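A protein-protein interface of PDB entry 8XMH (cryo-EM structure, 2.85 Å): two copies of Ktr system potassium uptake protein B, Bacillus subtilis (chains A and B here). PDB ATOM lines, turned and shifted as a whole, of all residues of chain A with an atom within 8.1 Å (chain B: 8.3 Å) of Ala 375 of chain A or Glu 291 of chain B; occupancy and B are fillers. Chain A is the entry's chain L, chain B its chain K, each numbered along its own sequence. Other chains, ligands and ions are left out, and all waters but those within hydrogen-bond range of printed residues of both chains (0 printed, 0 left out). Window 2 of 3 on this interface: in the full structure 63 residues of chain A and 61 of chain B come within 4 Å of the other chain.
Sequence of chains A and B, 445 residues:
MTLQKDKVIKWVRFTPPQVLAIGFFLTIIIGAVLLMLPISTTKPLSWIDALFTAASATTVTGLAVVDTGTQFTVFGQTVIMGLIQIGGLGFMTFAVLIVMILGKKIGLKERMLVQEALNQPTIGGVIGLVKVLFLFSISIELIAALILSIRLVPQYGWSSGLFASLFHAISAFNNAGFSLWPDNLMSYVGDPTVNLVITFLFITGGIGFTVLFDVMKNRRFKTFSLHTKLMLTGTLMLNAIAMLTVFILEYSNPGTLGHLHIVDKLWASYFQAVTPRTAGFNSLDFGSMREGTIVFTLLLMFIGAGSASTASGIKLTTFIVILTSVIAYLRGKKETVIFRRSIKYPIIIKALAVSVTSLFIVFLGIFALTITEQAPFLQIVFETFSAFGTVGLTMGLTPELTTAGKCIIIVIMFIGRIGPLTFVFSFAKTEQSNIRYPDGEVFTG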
ATOM      1  N   ILE A 366       8.945  22.284 -20.335  1.00  0.00           N
ATOM      2  CA  ILE A 366       7.526  22.012 -20.135  1.00  0.00           C
ATOM      3  C   ILE A 366       6.983  22.838 -18.976  1.00  0.00           C
ATOM      4  O   ILE A 366       5.857  23.347 -19.030  1.00  0.00           O
ATOM      5  CB  ILE A 366       7.301  20.504 -19.916  1.00  0.00           C
ATOM      6  CG1 ILE A 366       7.756  19.718 -21.143  1.00  0.00           C
ATOM      7  CG2 ILE A 366       5.845  20.208 -19.628  1.00  0.00           C
ATOM      8  CD1 ILE A 366       7.620  18.225 -20.994  1.00  0.00           C
ATOM      9  N   PHE A 367       7.771  22.983 -17.910  1.00  0.00           N
ATOM     10  CA  PHE A 367       7.343  23.787 -16.771  1.00  0.00           C
ATOM     11  C   PHE A 367       7.199  25.255 -17.151  1.00  0.00           C
ATOM     12  O   PHE A 367       6.253  25.923 -16.720  1.00  0.00           O
ATOM     13  CB  PHE A 367       8.332  23.620 -15.619  1.00  0.00           C
ATOM     14  CG  PHE A 367       7.948  24.365 -14.376  1.00  0.00           C
ATOM     15  CD1 PHE A 367       6.957  23.881 -13.542  1.00  0.00           C
ATOM     16  CD2 PHE A 367       8.586  25.544 -14.037  1.00  0.00           C
ATOM     17  CE1 PHE A 367       6.605  24.563 -12.397  1.00  0.00           C
ATOM     18  CE2 PHE A 367       8.238  26.230 -12.894  1.00  0.00           C
ATOM     19  CZ  PHE A 367       7.245  25.739 -12.073  1.00  0.00           C
ATOM     20  N   LEU A 369       6.666  26.474 -20.239  1.00  0.00           N
ATOM     21  CA  LEU A 369       5.625  26.674 -21.242  1.00  0.00           C
ATOM     22  C   LEU A 369       4.230  26.601 -20.639  1.00  0.00           C
ATOM     23  O   LEU A 369       3.315  27.279 -21.120  1.00  0.00           O
ATOM     24  CB  LEU A 369       5.764  25.648 -22.365  1.00  0.00           C
ATOM     25  CG  LEU A 369       6.806  25.934 -23.443  1.00  0.00           C
ATOM     26  CD1 LEU A 369       6.755  24.862 -24.511  1.00  0.00           C
ATOM     27  CD2 LEU A 369       6.571  27.300 -24.049  1.00  0.00           C
ATOM     28  N   THR A 370       4.037  25.781 -19.604  1.00  0.00           N
ATOM     29  CA  THR A 370       2.729  25.702 -18.964  1.00  0.00           C
ATOM     30  C   THR A 370       2.394  26.981 -18.210  1.00  0.00           C
ATOM     31  O   THR A 370       1.219  27.356 -18.124  1.00  0.00           O
ATOM     32  CB  THR A 370       2.674  24.503 -18.020  1.00  0.00           C
ATOM     33  OG1 THR A 370       3.861  24.468 -17.222  1.00  0.00           O
ATOM     34  CG2 THR A 370       2.554  23.211 -18.805  1.00  0.00           C
ATOM     35  N   ILE A 371       3.401  27.653 -17.651  1.00  0.00           N
ATOM     36  CA  ILE A 371       3.171  28.938 -17.000  1.00  0.00           C
ATOM     37  C   ILE A 371       2.762  29.989 -18.022  1.00  0.00           C
ATOM     38  O   ILE A 371       1.825  30.764 -17.799  1.00  0.00           O
ATOM     39  CB  ILE A 371       4.424  29.369 -16.216  1.00  0.00           C
ATOM     40  CG1 ILE A 371       4.771  28.335 -15.147  1.00  0.00           C
ATOM     41  CG2 ILE A 371       4.215  30.723 -15.573  1.00  0.00           C
ATOM     42  CD1 ILE A 371       3.678  28.117 -14.138  1.00  0.00           C
ATOM     43  N   THR A 372       3.443  30.023 -19.166  1.00  0.00           N
ATOM     44  CA  THR A 372       3.234  31.069 -20.160  1.00  0.00           C
ATOM     45  C   THR A 372       2.073  30.749 -21.100  1.00  0.00           C
ATOM     46  O   THR A 372       1.105  31.510 -21.183  1.00  0.00           O
ATOM     47  CB  THR A 372       4.518  31.284 -20.964  1.00  0.00           C
ATOM     48  OG1 THR A 372       5.600  31.570 -20.071  1.00  0.00           O
ATOM     49  CG2 THR A 372       4.347  32.440 -21.929  1.00  0.00           C
ATOM     50  N   GLU A 373       2.161  29.630 -21.810  1.00  0.00           N
ATOM     51  CA  GLU A 373       1.192  29.311 -22.847  1.00  0.00           C
ATOM     52  C   GLU A 373      -0.065  28.684 -22.261  1.00  0.00           C
ATOM     53  O   GLU A 373      -0.001  27.869 -21.338  1.00  0.00           O
ATOM     54  CB  GLU A 373       1.812  28.364 -23.874  1.00  0.00           C
ATOM     55  CG  GLU A 373       2.959  28.973 -24.649  1.00  0.00           C
ATOM     56  CD  GLU A 373       2.510  30.108 -25.545  1.00  0.00           C
ATOM     57  OE1 GLU A 373       1.389  30.029 -26.089  1.00  0.00           O
ATOM     58  OE2 GLU A 373       3.277  31.080 -25.701  1.00  0.00           O
ATOM     59  N   GLN A 374      -1.212  29.071 -22.812  1.00  0.00           N
ATOM     60  CA  GLN A 374      -2.500  28.472 -22.469  1.00  0.00           C
ATOM     61  C   GLN A 374      -2.845  27.486 -23.580  1.00  0.00           C
ATOM     62  O   GLN A 374      -3.495  27.843 -24.564  1.00  0.00           O
ATOM     63  CB  GLN A 374      -3.574  29.543 -22.308  1.00  0.00           C
ATOM     64  CG  GLN A 374      -3.224  30.622 -21.295  1.00  0.00           C
ATOM     65  CD  GLN A 374      -3.128  30.088 -19.879  1.00  0.00           C
ATOM     66  OE1 GLN A 374      -3.826  29.142 -19.511  1.00  0.00           O
ATOM     67  NE2 GLN A 374      -2.260  30.692 -19.076  1.00  0.00           N
ATOM     68  N   ALA A 375      -2.405  26.244 -23.416  1.00  0.00           N
ATOM     69  CA  ALA A 375      -2.515  25.231 -24.453  1.00  0.00           C
ATOM     70  C   ALA A 375      -2.806  23.896 -23.793  1.00  0.00           C
ATOM     71  O   ALA A 375      -2.575  23.734 -22.588  1.00  0.00           O
ATOM     72  CB  ALA A 375      -1.230  25.152 -25.286  1.00  0.00           C
ATOM     73  N   PRO A 376      -3.344  22.929 -24.539  1.00  0.00           N
ATOM     74  CA  PRO A 376      -3.457  21.570 -24.000  1.00  0.00           C
ATOM     75  C   PRO A 376      -2.093  21.000 -23.648  1.00  0.00           C
ATOM     76  O   PRO A 376      -1.086  21.291 -24.297  1.00  0.00           O
ATOM     77  CB  PRO A 376      -4.111  20.790 -25.145  1.00  0.00           C
ATOM     78  CG  PRO A 376      -4.881  21.812 -25.885  1.00  0.00           C
ATOM     79  CD  PRO A 376      -4.074  23.074 -25.810  1.00  0.00           C
ATOM     80  N   PHE A 377      -2.073  20.184 -22.592  1.00  0.00           N
ATOM     81  CA  PHE A 377      -0.813  19.693 -22.044  1.00  0.00           C
ATOM     82  C   PHE A 377      -0.092  18.764 -23.009  1.00  0.00           C
ATOM     83  O   PHE A 377       1.143  18.752 -23.041  1.00  0.00           O
ATOM     84  CB  PHE A 377      -1.070  18.986 -20.715  1.00  0.00           C
ATOM     85  CG  PHE A 377       0.168  18.476 -20.047  1.00  0.00           C
ATOM     86  CD1 PHE A 377       1.092  19.356 -19.514  1.00  0.00           C
ATOM     87  CD2 PHE A 377       0.399  17.117 -19.931  1.00  0.00           C
ATOM     88  CE1 PHE A 377       2.227  18.891 -18.894  1.00  0.00           C
ATOM     89  CE2 PHE A 377       1.532  16.647 -19.309  1.00  0.00           C
ATOM     90  CZ  PHE A 377       2.446  17.535 -18.787  1.00  0.00           C
ATOM     91  N   LEU A 378      -0.832  17.984 -23.799  1.00  0.00           N
ATOM     92  CA  LEU A 378      -0.195  17.075 -24.746  1.00  0.00           C
ATOM     93  C   LEU A 378       0.545  17.843 -25.833  1.00  0.00           C
ATOM     94  O   LEU A 378       1.603  17.405 -26.299  1.00  0.00           O
ATOM     95  CB  LEU A 378      -1.235  16.138 -25.356  1.00  0.00           C
ATOM     96  CG  LEU A 378      -0.727  15.056 -26.308  1.00  0.00           C
ATOM     97  CD1 LEU A 378       0.396  14.262 -25.674  1.00  0.00           C
ATOM     98  CD2 LEU A 378      -1.860  14.134 -26.717  1.00  0.00           C
ATOM     99  N   GLN A 379       0.008  18.991 -26.249  1.00  0.00           N
ATOM    100  CA  GLN A 379       0.689  19.804 -27.249  1.00  0.00           C
ATOM    101  C   GLN A 379       1.931  20.477 -26.683  1.00  0.00           C
ATOM    102  O   GLN A 379       2.906  20.681 -27.413  1.00  0.00           O
ATOM    103  CB  GLN A 379      -0.271  20.849 -27.811  1.00  0.00           C
ATOM    104  CG  GLN A 379      -1.494  20.250 -28.467  1.00  0.00           C
ATOM    105  CD  GLN A 379      -2.348  21.290 -29.148  1.00  0.00           C
ATOM    106  OE1 GLN A 379      -2.040  22.480 -29.116  1.00  0.00           O
ATOM    107  NE2 GLN A 379      -3.431  20.847 -29.773  1.00  0.00           N
ATOM    108  N   ILE A 380       1.912  20.836 -25.401  1.00  0.00           N
ATOM    109  CA  ILE A 380       3.071  21.470 -24.778  1.00  0.00           C
ATOM    110  C   ILE A 380       4.220  20.477 -24.639  1.00  0.00           C
ATOM    111  O   ILE A 380       5.382  20.812 -24.894  1.00  0.00           O
ATOM    112  CB  ILE A 380       2.669  22.083 -23.425  1.00  0.00           C
ATOM    113  CG1 ILE A 380       1.767  23.297 -23.644  1.00  0.00           C
ATOM    114  CG2 ILE A 380       3.887  22.470 -22.611  1.00  0.00           C
ATOM    115  CD1 ILE A 380       1.260  23.915 -22.367  1.00  0.00           C
ATOM    116  N   VAL A 381       3.917  19.244 -24.229  1.00  0.00           N
ATOM    117  CA  VAL A 381       4.959  18.230 -24.093  1.00  0.00           C
ATOM    118  C   VAL A 381       5.509  17.841 -25.459  1.00  0.00           C
ATOM    119  O   VAL A 381       6.718  17.650 -25.624  1.00  0.00           O
ATOM    120  CB  VAL A 381       4.415  17.010 -23.330  1.00  0.00           C
ATOM    121  CG1 VAL A 381       5.490  15.958 -23.166  1.00  0.00           C
ATOM    122  CG2 VAL A 381       3.903  17.435 -21.982  1.00  0.00           C
ATOM    123  N   GLY A 396       0.011  21.742 -33.573  1.00  0.00           N
ATOM    124  CA  GLY A 396      -0.792  22.935 -33.744  1.00  0.00           C
ATOM    125  C   GLY A 396      -0.543  23.985 -32.683  1.00  0.00           C
ATOM    126  O   GLY A 396      -1.458  24.724 -32.309  1.00  0.00           O
ATOM    127  N   LEU A 397       0.693  24.070 -32.197  1.00  0.00           N
ATOM    128  CA  LEU A 397       1.042  24.997 -31.128  1.00  0.00           C
ATOM    129  C   LEU A 397       1.983  26.109 -31.560  1.00  0.00           C
ATOM    130  O   LEU A 397       1.860  27.228 -31.056  1.00  0.00           O
ATOM    131  CB  LEU A 397       1.678  24.236 -29.957  1.00  0.00           C
ATOM    132  CG  LEU A 397       2.102  25.047 -28.730  1.00  0.00           C
ATOM    133  CD1 LEU A 397       0.926  25.834 -28.191  1.00  0.00           C
ATOM    134  CD2 LEU A 397       2.685  24.153 -27.655  1.00  0.00           C
ATOM    135  N   GLU A 400       0.558  29.332 -32.532  1.00  0.00           N
ATOM    136  CA  GLU A 400      -0.211  29.889 -31.427  1.00  0.00           C
ATOM    137  C   GLU A 400       0.655  30.344 -30.259  1.00  0.00           C
ATOM    138  O   GLU A 400       0.110  30.782 -29.241  1.00  0.00           O
ATOM    139  CB  GLU A 400      -1.233  28.860 -30.933  1.00  0.00           C
ATOM    140  CG  GLU A 400      -2.069  28.231 -32.036  1.00  0.00           C
ATOM    141  CD  GLU A 400      -3.030  29.211 -32.675  1.00  0.00           C
ATOM    142  OE1 GLU A 400      -3.461  30.162 -31.989  1.00  0.00           O
ATOM    143  OE2 GLU A 400      -3.356  29.031 -33.867  1.00  0.00           O
ATOM    144  N   LEU A 401       1.976  30.245 -30.372  1.00  0.00           N
ATOM    145  CA  LEU A 401       2.852  30.646 -29.279  1.00  0.00           C
ATOM    146  C   LEU A 401       2.842  32.158 -29.104  1.00  0.00           C
ATOM    147  O   LEU A 401       2.720  32.913 -30.071  1.00  0.00           O
ATOM    148  CB  LEU A 401       4.280  30.165 -29.534  1.00  0.00           C
ATOM    149  CG  LEU A 401       4.547  28.664 -29.458  1.00  0.00           C
ATOM    150  CD1 LEU A 401       5.988  28.367 -29.826  1.00  0.00           C
ATOM    151  CD2 LEU A 401       4.236  28.146 -28.070  1.00  0.00           C
ATOM    152  N   LEU B 249       2.475  29.979  -7.432  1.00  0.00           N
ATOM    153  CA  LEU B 249       1.734  29.624  -8.639  1.00  0.00           C
ATOM    154  C   LEU B 249       0.227  29.654  -8.411  1.00  0.00           C
ATOM    155  O   LEU B 249      -0.530  30.052  -9.304  1.00  0.00           O
ATOM    156  CB  LEU B 249       2.172  28.246  -9.135  1.00  0.00           C
ATOM    157  CG  LEU B 249       3.297  28.161 -10.171  1.00  0.00           C
ATOM    158  CD1 LEU B 249       4.599  28.751  -9.655  1.00  0.00           C
ATOM    159  CD2 LEU B 249       3.503  26.722 -10.587  1.00  0.00           C
ATOM    160  N   GLU B 250      -0.229  29.242  -7.230  1.00  0.00           N
ATOM    161  CA  GLU B 250      -1.650  29.105  -6.946  1.00  0.00           C
ATOM    162  C   GLU B 250      -2.232  30.296  -6.196  1.00  0.00           C
ATOM    163  O   GLU B 250      -3.383  30.229  -5.756  1.00  0.00           O
ATOM    164  CB  GLU B 250      -1.903  27.826  -6.147  1.00  0.00           C
ATOM    165  CG  GLU B 250      -1.513  26.555  -6.871  1.00  0.00           C
ATOM    166  CD  GLU B 250      -2.438  26.243  -8.023  1.00  0.00           C
ATOM    167  OE1 GLU B 250      -3.638  26.569  -7.923  1.00  0.00           O
ATOM    168  OE2 GLU B 250      -1.968  25.678  -9.030  1.00  0.00           O
ATOM    169  N   ASN B 253      -5.039  31.761  -8.281  1.00  0.00           N
ATOM    170  CA  ASN B 253      -5.953  30.761  -8.819  1.00  0.00           C
ATOM    171  C   ASN B 253      -7.309  30.877  -8.135  1.00  0.00           C
ATOM    172  O   ASN B 253      -7.373  30.840  -6.902  1.00  0.00           O
ATOM    173  CB  ASN B 253      -5.376  29.364  -8.627  1.00  0.00           C
ATOM    174  CG  ASN B 253      -6.242  28.285  -9.240  1.00  0.00           C
ATOM    175  OD1 ASN B 253      -7.092  27.701  -8.572  1.00  0.00           O
ATOM    176  ND2 ASN B 253      -6.029  28.015 -10.520  1.00  0.00           N
ATOM    177  N   PHE B 286      -6.974  19.080  -6.637  1.00  0.00           N
ATOM    178  CA  PHE B 286      -5.912  19.018  -7.633  1.00  0.00           C
ATOM    179  C   PHE B 286      -6.441  19.122  -9.055  1.00  0.00           C
ATOM    180  O   PHE B 286      -5.674  19.448  -9.966  1.00  0.00           O
ATOM    181  CB  PHE B 286      -5.108  17.729  -7.472  1.00  0.00           C
ATOM    182  CG  PHE B 286      -4.032  17.817  -6.436  1.00  0.00           C
ATOM    183  CD1 PHE B 286      -4.344  17.774  -5.090  1.00  0.00           C
ATOM    184  CD2 PHE B 286      -2.705  17.942  -6.807  1.00  0.00           C
ATOM    185  CE1 PHE B 286      -3.355  17.857  -4.133  1.00  0.00           C
ATOM    186  CE2 PHE B 286      -1.711  18.023  -5.856  1.00  0.00           C
ATOM    187  CZ  PHE B 286      -2.037  17.981  -4.518  1.00  0.00           C
ATOM    188  N   GLY B 287      -7.731  18.858  -9.268  1.00  0.00           N
ATOM    189  CA  GLY B 287      -8.295  18.979 -10.599  1.00  0.00           C
ATOM    190  C   GLY B 287      -8.468  20.407 -11.065  1.00  0.00           C
ATOM    191  O   GLY B 287      -8.547  20.648 -12.273  1.00  0.00           O
ATOM    192  N   SER B 288      -8.532  21.359 -10.137  1.00  0.00           N
ATOM    193  CA  SER B 288      -8.703  22.765 -10.469  1.00  0.00           C
ATOM    194  C   SER B 288      -7.416  23.570 -10.352  1.00  0.00           C
ATOM    195  O   SER B 288      -7.454  24.794 -10.502  1.00  0.00           O
ATOM    196  CB  SER B 288      -9.784  23.386  -9.577  1.00  0.00           C
ATOM    197  OG  SER B 288      -9.513  23.144  -8.210  1.00  0.00           O
ATOM    198  N   MET B 289      -6.286  22.922 -10.088  1.00  0.00           N
ATOM    199  CA  MET B 289      -5.017  23.629 -10.041  1.00  0.00           C
ATOM    200  C   MET B 289      -4.524  23.939 -11.450  1.00  0.00           C
ATOM    201  O   MET B 289      -4.969  23.352 -12.439  1.00  0.00           O
ATOM    202  CB  MET B 289      -3.964  22.812  -9.295  1.00  0.00           C
ATOM    203  CG  MET B 289      -4.200  22.703  -7.804  1.00  0.00           C
ATOM    204  SD  MET B 289      -2.848  21.868  -6.958  1.00  0.00           S
ATOM    205  CE  MET B 289      -3.428  21.931  -5.266  1.00  0.00           C
ATOM    206  N   ARG B 290      -3.591  24.882 -11.529  1.00  0.00           N
ATOM    207  CA  ARG B 290      -2.983  25.223 -12.802  1.00  0.00           C
ATOM    208  C   ARG B 290      -2.062  24.099 -13.269  1.00  0.00           C
ATOM    209  O   ARG B 290      -1.634  23.244 -12.490  1.00  0.00           O
ATOM    210  CB  ARG B 290      -2.205  26.533 -12.691  1.00  0.00           C
ATOM    211  CG  ARG B 290      -3.073  27.738 -12.374  1.00  0.00           C
ATOM    212  CD  ARG B 290      -2.321  29.035 -12.615  1.00  0.00           C
ATOM    213  NE  ARG B 290      -3.194  30.199 -12.530  1.00  0.00           N
ATOM    214  CZ  ARG B 290      -3.286  30.990 -11.472  1.00  0.00           C
ATOM    215  NH1 ARG B 290      -2.563  30.778 -10.386  1.00  0.00           N
ATOM    216  NH2 ARG B 290      -4.123  32.024 -11.505  1.00  0.00           N
ATOM    217  N   GLU B 291      -1.765  24.104 -14.570  1.00  0.00           N
ATOM    218  CA  GLU B 291      -0.903  23.070 -15.132  1.00  0.00           C
ATOM    219  C   GLU B 291       0.533  23.200 -14.643  1.00  0.00           C
ATOM    220  O   GLU B 291       1.263  22.205 -14.613  1.00  0.00           O
ATOM    221  CB  GLU B 291      -0.946  23.118 -16.659  1.00  0.00           C
ATOM    222  CG  GLU B 291      -2.294  22.752 -17.256  1.00  0.00           C
ATOM    223  CD  GLU B 291      -2.276  22.740 -18.772  1.00  0.00           C
ATOM    224  OE1 GLU B 291      -1.250  23.145 -19.357  1.00  0.00           O
ATOM    225  OE2 GLU B 291      -3.286  22.326 -19.379  1.00  0.00           O
ATOM    226  N   GLY B 292       0.958  24.409 -14.269  1.00  0.00           N
ATOM    227  CA  GLY B 292       2.320  24.590 -13.794  1.00  0.00           C
ATOM    228  C   GLY B 292       2.586  23.897 -12.472  1.00  0.00           C
ATOM    229  O   GLY B 292       3.666  23.344 -12.260  1.00  0.00           O
ATOM    230  N   THR B 293       1.612  23.929 -11.560  1.00  0.00           N
ATOM    231  CA  THR B 293       1.782  23.267 -10.271  1.00  0.00           C
ATOM    232  C   THR B 293       1.747  21.751 -10.410  1.00  0.00           C
ATOM    233  O   THR B 293       2.441  21.045  -9.671  1.00  0.00           O
ATOM    234  CB  THR B 293       0.698  23.730  -9.298  1.00  0.00           C
ATOM    235  OG1 THR B 293       0.545  25.149  -9.394  1.00  0.00           O
ATOM    236  CG2 THR B 293       1.074  23.374  -7.871  1.00  0.00           C
ATOM    237  N   ILE B 294       0.946  21.242 -11.345  1.00  0.00           N
ATOM    238  CA  ILE B 294       0.841  19.802 -11.551  1.00  0.00           C
ATOM    239  C   ILE B 294       2.138  19.243 -12.125  1.00  0.00           C
ATOM    240  O   ILE B 294       2.555  18.131 -11.782  1.00  0.00           O
ATOM    241  CB  ILE B 294      -0.371  19.499 -12.450  1.00  0.00           C
ATOM    242  CG1 ILE B 294      -1.654  19.964 -11.758  1.00  0.00           C
ATOM    243  CG2 ILE B 294      -0.457  18.027 -12.781  1.00  0.00           C
ATOM    244  CD1 ILE B 294      -2.875  19.905 -12.634  1.00  0.00           C
ATOM    245  N   VAL B 295       2.795  20.001 -13.006  1.00  0.00           N
ATOM    246  CA  VAL B 295       4.079  19.572 -13.555  1.00  0.00           C
ATOM    247  C   VAL B 295       5.130  19.483 -12.456  1.00  0.00           C
ATOM    248  O   VAL B 295       5.906  18.522 -12.394  1.00  0.00           O
ATOM    249  CB  VAL B 295       4.516  20.520 -14.688  1.00  0.00           C
ATOM    250  CG1 VAL B 295       5.954  20.257 -15.091  1.00  0.00           C
ATOM    251  CG2 VAL B 295       3.604  20.349 -15.880  1.00  0.00           C
ATOM    252  N   PHE B 296       5.167  20.476 -11.566  1.00  0.00           N
ATOM    253  CA  PHE B 296       6.106  20.422 -10.453  1.00  0.00           C
ATOM    254  C   PHE B 296       5.751  19.315  -9.471  1.00  0.00           C
ATOM    255  O   PHE B 296       6.647  18.719  -8.863  1.00  0.00           O
ATOM    256  CB  PHE B 296       6.156  21.771  -9.741  1.00  0.00           C
ATOM    257  CG  PHE B 296       7.146  21.821  -8.620  1.00  0.00           C
ATOM    258  CD1 PHE B 296       8.496  21.969  -8.880  1.00  0.00           C
ATOM    259  CD2 PHE B 296       6.727  21.721  -7.305  1.00  0.00           C
ATOM    260  CE1 PHE B 296       9.410  22.011  -7.850  1.00  0.00           C
ATOM    261  CE2 PHE B 296       7.635  21.762  -6.274  1.00  0.00           C
ATOM    262  CZ  PHE B 296       8.978  21.908  -6.546  1.00  0.00           C
ATOM    263  N   THR B 297       4.459  19.031  -9.296  1.00  0.00           N
ATOM    264  CA  THR B 297       4.050  17.927  -8.436  1.00  0.00           C
ATOM    265  C   THR B 297       4.434  16.580  -9.035  1.00  0.00           C
ATOM    266  O   THR B 297       4.704  15.631  -8.293  1.00  0.00           O
ATOM    267  CB  THR B 297       2.543  17.991  -8.187  1.00  0.00           C
ATOM    268  OG1 THR B 297       2.181  19.328  -7.829  1.00  0.00           O
ATOM    269  CG2 THR B 297       2.138  17.063  -7.060  1.00  0.00           C
ATOM    270  N   LEU B 298       4.461  16.484 -10.358  1.00  0.00           N
ATOM    271  CA  LEU B 298       4.868  15.239 -11.001  1.00  0.00           C
ATOM    272  C   LEU B 298       6.298  14.887 -10.617  1.00  0.00           C
ATOM    273  O   LEU B 298       6.572  13.751 -10.229  1.00  0.00           O
ATOM    274  CB  LEU B 298       4.728  15.343 -12.517  1.00  0.00           C
ATOM    275  CG  LEU B 298       3.507  14.631 -13.101  1.00  0.00           C
ATOM    276  CD1 LEU B 298       2.215  15.092 -12.451  1.00  0.00           C
ATOM    277  CD2 LEU B 298       3.447  14.858 -14.600  1.00  0.00           C
ATOM    278  N   LEU B 378      -3.141  15.026 -19.272  1.00  0.00           N
ATOM    279  CA  LEU B 378      -2.571  15.463 -18.003  1.00  0.00           C
ATOM    280  C   LEU B 378      -3.066  14.601 -16.849  1.00  0.00           C
ATOM    281  O   LEU B 378      -2.319  14.336 -15.901  1.00  0.00           O
ATOM    282  CB  LEU B 378      -2.899  16.935 -17.760  1.00  0.00           C
ATOM    283  CG  LEU B 378      -2.304  17.588 -16.511  1.00  0.00           C
ATOM    284  CD1 LEU B 378      -0.807  17.359 -16.446  1.00  0.00           C
ATOM    285  CD2 LEU B 378      -2.613  19.072 -16.491  1.00  0.00           C
ATOM    286  N   MET B 395      -6.718  13.675 -10.074  1.00  0.00           N
ATOM    287  CA  MET B 395      -7.330  14.814 -10.735  1.00  0.00           C
ATOM    288  C   MET B 395      -8.742  14.516 -11.217  1.00  0.00           C
ATOM    289  O   MET B 395      -9.352  15.368 -11.870  1.00  0.00           O
ATOM    290  CB  MET B 395      -6.463  15.274 -11.910  1.00  0.00           C
ATOM    291  CG  MET B 395      -5.142  15.889 -11.496  1.00  0.00           C
ATOM    292  SD  MET B 395      -4.159  16.405 -12.911  1.00  0.00           S
ATOM    293  CE  MET B 395      -5.346  17.417 -13.787  1.00  0.00           C
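Hydrophobic or aromatic side chains of chain A that line the printed part of chain B: Phe 367, Ile 371, Phe 377 and Ile 380. Of the 18 printed residues of chain B, 6 touch a printed residue of chain A. Hydrophobic or aromatic side chains of chain B that line the printed part of chain A: Leu 249, Val 295, Phe 296 and Leu 378.
Among the printed residues, pairs that only touch across the chains: Phe 367 of chain A with Gly 292 of chain B, Ala 375 of chain A with Glu 291 of chain B, Phe 377 of chain A with Val 295 of chain B, Phe 377 of chain A with Leu 378 of chain B, Thr 370 of chain A with Gly 292 of chain B, Ile 371 of chain A with Gly 292 of chain B, Ile 371 of chain A with Leu 249 of chain B, Thr 370 of chain A with Glu 291 of chain B, Phe 367 of chain A with Phe 296 of chain B and Ile 380 of chain A with Glu 291 of chain B.
O of Leu 249 of chain B is in hydrogen-bond range of NH1 of Arg 290 of chain B (2.4 Å). OG1 of Thr 370 of chain A is in hydrogen-bond range of O of Ile 366 of chain A. The backbone carbonyl oxygen (O) of Phe 367 of chain A lies within hydrogen-bond range of the side-chain hydroxyl (OG1) of Thr 370 of chain A (2.8 Å).
1 position is printed for both chains.
Of the printed residues of chain B, Phe 367 of chain A touches Gly 292 (3.2 Å) and Phe 296 (3.9 Å). Of the printed residues of chain B, Ile 371 of chain A touches Leu 249 (3.8 Å) and Gly 292 (3.8 Å). Printed residues of chain B within 4 Å of Ala 375 of chain A: Glu 291. No residue of chain B comes within 4 Å of Pro 376 of chain A. Printed residues of chain B within 4 Å of Ile 380 of chain A: Glu 291 (3.99 Å). Of the printed residues of chain A, Gly 292 of chain B touches Phe 367, Thr 370 and Ile 371. Printed residues of chain A within 4 Å of Leu 378 of chain B: Phe 377 (3.7 Å). The nearest printed residue of chain A that does not touch Glu 291 of chain B is Phe 377 of chain A (4.05 Å).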
